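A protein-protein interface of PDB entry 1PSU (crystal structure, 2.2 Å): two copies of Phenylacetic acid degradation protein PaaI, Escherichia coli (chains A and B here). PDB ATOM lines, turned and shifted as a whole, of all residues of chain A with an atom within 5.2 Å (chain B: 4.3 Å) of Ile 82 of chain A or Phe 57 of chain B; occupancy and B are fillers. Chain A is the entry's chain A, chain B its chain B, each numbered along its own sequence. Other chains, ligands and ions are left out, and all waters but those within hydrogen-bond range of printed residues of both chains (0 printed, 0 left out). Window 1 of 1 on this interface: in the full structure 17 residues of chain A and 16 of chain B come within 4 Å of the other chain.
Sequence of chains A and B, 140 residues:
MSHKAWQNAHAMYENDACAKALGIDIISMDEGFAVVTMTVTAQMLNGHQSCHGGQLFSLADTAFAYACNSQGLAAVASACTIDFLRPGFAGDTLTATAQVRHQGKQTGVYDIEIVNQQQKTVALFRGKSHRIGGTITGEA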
ATOM      1  N   GLY A  53      11.231  -4.558  -6.349  1.00  0.00           N
ATOM      2  CA  GLY A  53       9.958  -3.871  -6.491  1.00  0.00           C
ATOM      3  C   GLY A  53       8.908  -4.588  -7.318  1.00  0.00           C
ATOM      4  O   GLY A  53       7.721  -4.469  -7.043  1.00  0.00           O
ATOM      5  N   GLY A  54       9.343  -5.337  -8.325  1.00  0.00           N
ATOM      6  CA  GLY A  54       8.411  -6.044  -9.183  1.00  0.00           C
ATOM      7  C   GLY A  54       7.606  -7.096  -8.456  1.00  0.00           C
ATOM      8  O   GLY A  54       6.424  -7.293  -8.750  1.00  0.00           O
ATOM      9  N   PHE A  57       5.149  -5.339  -6.187  1.00  0.00           N
ATOM     10  CA  PHE A  57       4.035  -4.827  -6.965  1.00  0.00           C
ATOM     11  C   PHE A  57       3.060  -5.966  -7.249  1.00  0.00           C
ATOM     12  O   PHE A  57       1.850  -5.814  -7.082  1.00  0.00           O
ATOM     13  CB  PHE A  57       4.543  -4.216  -8.275  1.00  0.00           C
ATOM     14  CG  PHE A  57       3.467  -3.568  -9.095  1.00  0.00           C
ATOM     15  CD1 PHE A  57       3.200  -2.211  -8.966  1.00  0.00           C
ATOM     16  CD2 PHE A  57       2.697  -4.322  -9.975  1.00  0.00           C
ATOM     17  CE1 PHE A  57       2.180  -1.612  -9.700  1.00  0.00           C
ATOM     18  CE2 PHE A  57       1.673  -3.733 -10.715  1.00  0.00           C
ATOM     19  CZ  PHE A  57       1.416  -2.372 -10.576  1.00  0.00           C
ATOM     20  N   CYS A  80      -0.941   4.057  -9.967  1.00  0.00           N
ATOM     21  CA  CYS A  80      -0.567   3.572  -8.641  1.00  0.00           C
ATOM     22  C   CYS A  80       0.607   4.362  -8.092  1.00  0.00           C
ATOM     23  O   CYS A  80       1.517   4.726  -8.829  1.00  0.00           O
ATOM     24  CB  CYS A  80      -0.194   2.087  -8.693  1.00  0.00           C
ATOM     25  SG  CYS A  80       0.098   1.390  -7.034  1.00  0.00           S
ATOM     26  N   THR A  81       0.565   4.638  -6.795  1.00  0.00           N
ATOM     27  CA  THR A  81       1.647   5.351  -6.135  1.00  0.00           C
ATOM     28  C   THR A  81       2.162   4.393  -5.079  1.00  0.00           C
ATOM     29  O   THR A  81       1.377   3.702  -4.444  1.00  0.00           O
ATOM     30  CB  THR A  81       1.170   6.645  -5.465  1.00  0.00           C
ATOM     31  OG1 THR A  81       0.634   7.518  -6.461  1.00  0.00           O
ATOM     32  CG2 THR A  81       2.339   7.352  -4.794  1.00  0.00           C
ATOM     33  N   ILE A  82       3.478   4.339  -4.902  1.00  0.00           N
ATOM     34  CA  ILE A  82       4.074   3.407  -3.954  1.00  0.00           C
ATOM     35  C   ILE A  82       5.156   4.062  -3.113  1.00  0.00           C
ATOM     36  O   ILE A  82       5.977   4.799  -3.634  1.00  0.00           O
ATOM     37  CB  ILE A  82       4.724   2.226  -4.702  1.00  0.00           C
ATOM     38  CG1 ILE A  82       3.794   1.741  -5.807  1.00  0.00           C
ATOM     39  CG2 ILE A  82       5.052   1.109  -3.714  1.00  0.00           C
ATOM     40  CD1 ILE A  82       4.430   0.724  -6.731  1.00  0.00           C
ATOM     41  N   ASP A  83       5.131   3.800  -1.809  1.00  0.00           N
ATOM     42  CA  ASP A  83       6.143   4.308  -0.896  1.00  0.00           C
ATOM     43  C   ASP A  83       6.849   3.093  -0.320  1.00  0.00           C
ATOM     44  O   ASP A  83       6.209   2.240   0.291  1.00  0.00           O
ATOM     45  CB  ASP A  83       5.518   5.112   0.248  1.00  0.00           C
ATOM     46  CG  ASP A  83       5.020   6.467  -0.201  1.00  0.00           C
ATOM     47  OD1 ASP A  83       5.840   7.294  -0.659  1.00  0.00           O
ATOM     48  OD2 ASP A  83       3.802   6.724  -0.093  1.00  0.00           O
ATOM     49  N   PHE A  84       8.158   2.991  -0.525  1.00  0.00           N
ATOM     50  CA  PHE A  84       8.917   1.865   0.027  1.00  0.00           C
ATOM     51  C   PHE A  84       9.510   2.348   1.335  1.00  0.00           C
ATOM     52  O   PHE A  84      10.298   3.296   1.352  1.00  0.00           O
ATOM     53  CB  PHE A  84      10.043   1.456  -0.912  1.00  0.00           C
ATOM     54  CG  PHE A  84       9.571   1.067  -2.274  1.00  0.00           C
ATOM     55  CD1 PHE A  84       9.490   2.014  -3.289  1.00  0.00           C
ATOM     56  CD2 PHE A  84       9.196  -0.248  -2.544  1.00  0.00           C
ATOM     57  CE1 PHE A  84       9.047   1.659  -4.570  1.00  0.00           C
ATOM     58  CE2 PHE A  84       8.749  -0.623  -3.821  1.00  0.00           C
ATOM     59  CZ  PHE A  84       8.674   0.334  -4.837  1.00  0.00           C
ATOM     60  N   ALA A 123       5.747  -1.524   2.683  1.00  0.00           N
ATOM     61  CA  ALA A 123       5.377  -0.611   1.622  1.00  0.00           C
ATOM     62  C   ALA A 123       3.903  -0.221   1.677  1.00  0.00           C
ATOM     63  O   ALA A 123       3.080  -0.967   2.184  1.00  0.00           O
ATOM     64  CB  ALA A 123       5.708  -1.233   0.281  1.00  0.00           C
ATOM     65  N   LEU A 124       3.594   0.966   1.165  1.00  0.00           N
ATOM     66  CA  LEU A 124       2.231   1.490   1.115  1.00  0.00           C
ATOM     67  C   LEU A 124       1.889   1.763  -0.333  1.00  0.00           C
ATOM     68  O   LEU A 124       2.660   2.411  -1.043  1.00  0.00           O
ATOM     69  CB  LEU A 124       2.120   2.796   1.907  1.00  0.00           C
ATOM     70  CG  LEU A 124       2.414   2.656   3.400  1.00  0.00           C
ATOM     71  CD1 LEU A 124       2.509   4.033   4.044  1.00  0.00           C
ATOM     72  CD2 LEU A 124       1.324   1.822   4.047  1.00  0.00           C
ATOM     73  N   PHE A 125       0.741   1.253  -0.767  1.00  0.00           N
ATOM     74  CA  PHE A 125       0.272   1.453  -2.130  1.00  0.00           C
ATOM     75  C   PHE A 125      -1.078   2.149  -2.124  1.00  0.00           C
ATOM     76  O   PHE A 125      -1.888   1.964  -1.218  1.00  0.00           O
ATOM     77  CB  PHE A 125       0.046   0.126  -2.864  1.00  0.00           C
ATOM     78  CG  PHE A 125       1.281  -0.686  -3.076  1.00  0.00           C
ATOM     79  CD1 PHE A 125       1.938  -1.284  -2.003  1.00  0.00           C
ATOM     80  CD2 PHE A 125       1.762  -0.895  -4.364  1.00  0.00           C
ATOM     81  CE1 PHE A 125       3.068  -2.088  -2.211  1.00  0.00           C
ATOM     82  CE2 PHE A 125       2.893  -1.698  -4.592  1.00  0.00           C
ATOM     83  CZ  PHE A 125       3.544  -2.296  -3.513  1.00  0.00           C
ATOM     84  N   GLY B  53       0.774  -5.923 -14.957  1.00  0.00           N
ATOM     85  CA  GLY B  53       1.344  -4.715 -14.383  1.00  0.00           C
ATOM     86  C   GLY B  53       2.696  -4.970 -13.740  1.00  0.00           C
ATOM     87  O   GLY B  53       3.605  -4.148 -13.837  1.00  0.00           O
ATOM     88  N   GLY B  54       2.833  -6.117 -13.089  1.00  0.00           N
ATOM     89  CA  GLY B  54       4.083  -6.445 -12.441  1.00  0.00           C
ATOM     90  C   GLY B  54       5.252  -6.429 -13.393  1.00  0.00           C
ATOM     91  O   GLY B  54       6.336  -5.973 -13.031  1.00  0.00           O
ATOM     92  N   GLN B  55       5.040  -6.929 -14.608  1.00  0.00           N
ATOM     93  CA  GLN B  55       6.099  -6.955 -15.625  1.00  0.00           C
ATOM     94  C   GLN B  55       6.421  -5.557 -16.161  1.00  0.00           C
ATOM     95  O   GLN B  55       7.578  -5.250 -16.411  1.00  0.00           O
ATOM     96  CB  GLN B  55       5.711  -7.888 -16.786  1.00  0.00           C
ATOM     97  CG  GLN B  55       6.026  -9.368 -16.533  1.00  0.00           C
ATOM     98  CD  GLN B  55       4.924 -10.116 -15.784  1.00  0.00           C
ATOM     99  OE1 GLN B  55       4.089  -9.513 -15.108  1.00  0.00           O
ATOM    100  NE2 GLN B  55       4.930 -11.444 -15.897  1.00  0.00           N
ATOM    101  N   LEU B  56       5.400  -4.723 -16.341  1.00  0.00           N
ATOM    102  CA  LEU B  56       5.627  -3.372 -16.819  1.00  0.00           C
ATOM    103  C   LEU B  56       6.346  -2.582 -15.734  1.00  0.00           C
ATOM    104  O   LEU B  56       7.231  -1.783 -16.024  1.00  0.00           O
ATOM    105  CB  LEU B  56       4.319  -2.670 -17.160  1.00  0.00           C
ATOM    106  CG  LEU B  56       3.621  -3.102 -18.441  1.00  0.00           C
ATOM    107  CD1 LEU B  56       2.453  -2.158 -18.706  1.00  0.00           C
ATOM    108  CD2 LEU B  56       4.598  -3.072 -19.610  1.00  0.00           C
ATOM    109  N   PHE B  57       5.960  -2.803 -14.482  1.00  0.00           N
ATOM    110  CA  PHE B  57       6.592  -2.107 -13.376  1.00  0.00           C
ATOM    111  C   PHE B  57       8.069  -2.479 -13.376  1.00  0.00           C
ATOM    112  O   PHE B  57       8.937  -1.621 -13.273  1.00  0.00           O
ATOM    113  CB  PHE B  57       5.966  -2.517 -12.038  1.00  0.00           C
ATOM    114  CG  PHE B  57       6.563  -1.802 -10.854  1.00  0.00           C
ATOM    115  CD1 PHE B  57       6.138  -0.526 -10.513  1.00  0.00           C
ATOM    116  CD2 PHE B  57       7.620  -2.359 -10.149  1.00  0.00           C
ATOM    117  CE1 PHE B  57       6.754   0.182  -9.489  1.00  0.00           C
ATOM    118  CE2 PHE B  57       8.244  -1.657  -9.122  1.00  0.00           C
ATOM    119  CZ  PHE B  57       7.810  -0.383  -8.798  1.00  0.00           C
ATOM    120  N   SER B  58       8.345  -3.768 -13.508  1.00  0.00           N
ATOM    121  CA  SER B  58       9.719  -4.258 -13.504  1.00  0.00           C
ATOM    122  C   SER B  58      10.572  -3.660 -14.602  1.00  0.00           C
ATOM    123  O   SER B  58      11.777  -3.437 -14.413  1.00  0.00           O
ATOM    124  CB  SER B  58       9.734  -5.772 -13.632  1.00  0.00           C
ATOM    125  OG  SER B  58       9.072  -6.353 -12.530  1.00  0.00           O
ATOM    126  N   LEU B  59       9.964  -3.418 -15.761  1.00  0.00           N
ATOM    127  CA  LEU B  59      10.685  -2.825 -16.882  1.00  0.00           C
ATOM    128  C   LEU B  59      11.036  -1.367 -16.580  1.00  0.00           C
ATOM    129  O   LEU B  59      12.155  -0.925 -16.838  1.00  0.00           O
ATOM    130  CB  LEU B  59       9.838  -2.894 -18.159  1.00  0.00           C
ATOM    131  CG  LEU B  59      10.487  -2.310 -19.418  1.00  0.00           C
ATOM    132  CD1 LEU B  59      11.668  -3.179 -19.839  1.00  0.00           C
ATOM    133  CD2 LEU B  59       9.470  -2.235 -20.557  1.00  0.00           C
ATOM    134  N   ALA B  60      10.074  -0.623 -16.040  1.00  0.00           N
ATOM    135  CA  ALA B  60      10.305   0.774 -15.720  1.00  0.00           C
ATOM    136  C   ALA B  60      11.316   0.882 -14.574  1.00  0.00           C
ATOM    137  O   ALA B  60      12.184   1.741 -14.585  1.00  0.00           O
ATOM    138  CB  ALA B  60       8.979   1.451 -15.330  1.00  0.00           C
ATOM    139  N   ASP B  61      11.207  -0.010 -13.599  1.00  0.00           N
ATOM    140  CA  ASP B  61      12.082   0.006 -12.440  1.00  0.00           C
ATOM    141  C   ASP B  61      13.516  -0.327 -12.839  1.00  0.00           C
ATOM    142  O   ASP B  61      14.469   0.117 -12.201  1.00  0.00           O
ATOM    143  CB  ASP B  61      11.563  -0.982 -11.391  1.00  0.00           C
ATOM    144  CG  ASP B  61      12.150  -0.738 -10.015  1.00  0.00           C
ATOM    145  OD1 ASP B  61      12.059   0.411  -9.517  1.00  0.00           O
ATOM    146  OD2 ASP B  61      12.677  -1.697  -9.406  1.00  0.00           O
ATOM    147  N   ALA B  79      10.235   5.772  -3.449  1.00  0.00           N
ATOM    148  CA  ALA B  79       8.848   5.992  -3.835  1.00  0.00           C
ATOM    149  C   ALA B  79       8.732   6.067  -5.339  1.00  0.00           C
ATOM    150  O   ALA B  79       9.713   6.326  -6.032  1.00  0.00           O
ATOM    151  CB  ALA B  79       8.338   7.290  -3.206  1.00  0.00           C
ATOM    152  N   CYS B  80       7.528   5.839  -5.848  1.00  0.00           N
ATOM    153  CA  CYS B  80       7.324   5.917  -7.274  1.00  0.00           C
ATOM    154  C   CYS B  80       5.851   5.906  -7.637  1.00  0.00           C
ATOM    155  O   CYS B  80       5.028   5.391  -6.894  1.00  0.00           O
ATOM    156  CB  CYS B  80       8.053   4.775  -7.981  1.00  0.00           C
ATOM    157  SG  CYS B  80       7.316   3.180  -7.811  1.00  0.00           S
ATOM    158  N   PHE B 125       6.137   6.725 -15.708  1.00  0.00           N
ATOM    159  CA  PHE B 125       6.605   6.380 -14.381  1.00  0.00           C
ATOM    160  C   PHE B 125       7.413   7.530 -13.802  1.00  0.00           C
ATOM    161  O   PHE B 125       8.029   8.285 -14.533  1.00  0.00           O
ATOM    162  CB  PHE B 125       7.480   5.141 -14.554  1.00  0.00           C
ATOM    163  CG  PHE B 125       8.083   4.610 -13.296  1.00  0.00           C
ATOM    164  CD1 PHE B 125       7.521   3.502 -12.679  1.00  0.00           C
ATOM    165  CD2 PHE B 125       9.266   5.146 -12.780  1.00  0.00           C
ATOM    166  CE1 PHE B 125       8.119   2.930 -11.561  1.00  0.00           C
ATOM    167  CE2 PHE B 125       9.876   4.582 -11.656  1.00  0.00           C
ATOM    168  CZ  PHE B 125       9.302   3.469 -11.053  1.00  0.00           C
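Of the 12 printed residues of chain B, 6 touch a printed residue of chain A. Hydrophobic or aromatic side chains of chain B that line the printed part of chain A: Phe 57 and Ala 79. Printed residues of chain A that touch a printed residue of chain B: Gly 53, Gly 54, Phe 57, Thr 81, Ile 82, Asp 83 and Phe 84.
The backbone carbonyl oxygen of Cys 80 of chain B is in hydrogen-bond range of the backbone NH of Ile 82 of chain A (2.7 Å).
Among the printed residues, merely in contact across the chains: Ile 82 of chain A with Ala 79 of chain B (3.1 Å), Phe 57 of chain A with Gly 53 of chain B (3.4 Å), Gly 54 of chain A with Ser 58 of chain B (3.4 Å), Thr 81 of chain A with Cys 80 of chain B (3.5 Å), Gly 53 of chain A with Phe 57 of chain B (3.5 Å), Phe 57 of chain A with Gly 54 of chain B (3.5 Å), Asp 83 of chain A with Ala 79 of chain B (3.6 Å), Ile 82 of chain A with Phe 57 of chain B (3.6 Å), Phe 57 of chain A with Phe 57 of chain B (3.7 Å), Phe 84 of chain A with Ala 79 of chain B (3.8 Å), Gly 54 of chain A with Phe 57 of chain B (3.9 Å) and Phe 84 of chain A with Cys 80 of chain B (3.98 Å).
N of Asp 83 of chain A lies within hydrogen-bond range of O of Leu 124 of chain A, 2.9 Å away. OG of Ser 58 of chain B is in hydrogen-bond range of O of Gly 54 of chain B (2.8 Å).
Gly 53 of chain A touches Phe 57 of chain B, and with the chains exchanged Phe 57 of chain A touches Gly 53 of chain B. Gly 54 of chain A touches Phe 57 of chain B, and with the chains exchanged Phe 57 of chain A touches Gly 54 of chain B. Phe 57 of chain A touches its own counterpart, Phe 57 of chain B. 5 positions are printed for both chains.
Printed residues of chain B within 4 Å of Gly 54 of chain A: Phe 57 (3.9 Å) and Ser 58 (3.4 Å). Of the printed residues of chain B, Phe 57 of chain A touches Gly 53 (3.4 Å), Gly 54 (3.5 Å) and Phe 57 (3.7 Å). Of chain B, only Phe 57 (3.6 Å), Ala 79 (3.1 Å) and Cys 80 (2.7 Å) come within 4 Å of Ile 82 of chain A. Of the printed residues of chain B, Phe 84 of chain A touches Ala 79 (3.8 Å) and Cys 80 (3.98 Å). Of chain A, only Gly 53, Gly 54, Phe 57 and Ile 82 come within 4 Å of Phe 57 of chain B. Printed residues of chain A within 4 Å of Ser 58 of chain B: Gly 54. Leu 59 of chain B touches none of the printed residues of chain A. Of the printed residues of chain A, Cys 80 of chain B touches Thr 81, Ile 82 and Phe 84. Phe 125 of chain B touches none of the printed residues of chain A. The nearest printed residue of chain B that does not touch Ile 82 of chain A is Phe 125 of chain B (6.5 Å). The nearest printed residue of chain B that does not touch Phe 84 of chain A is Phe 57 of chain B (4.1 Å).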
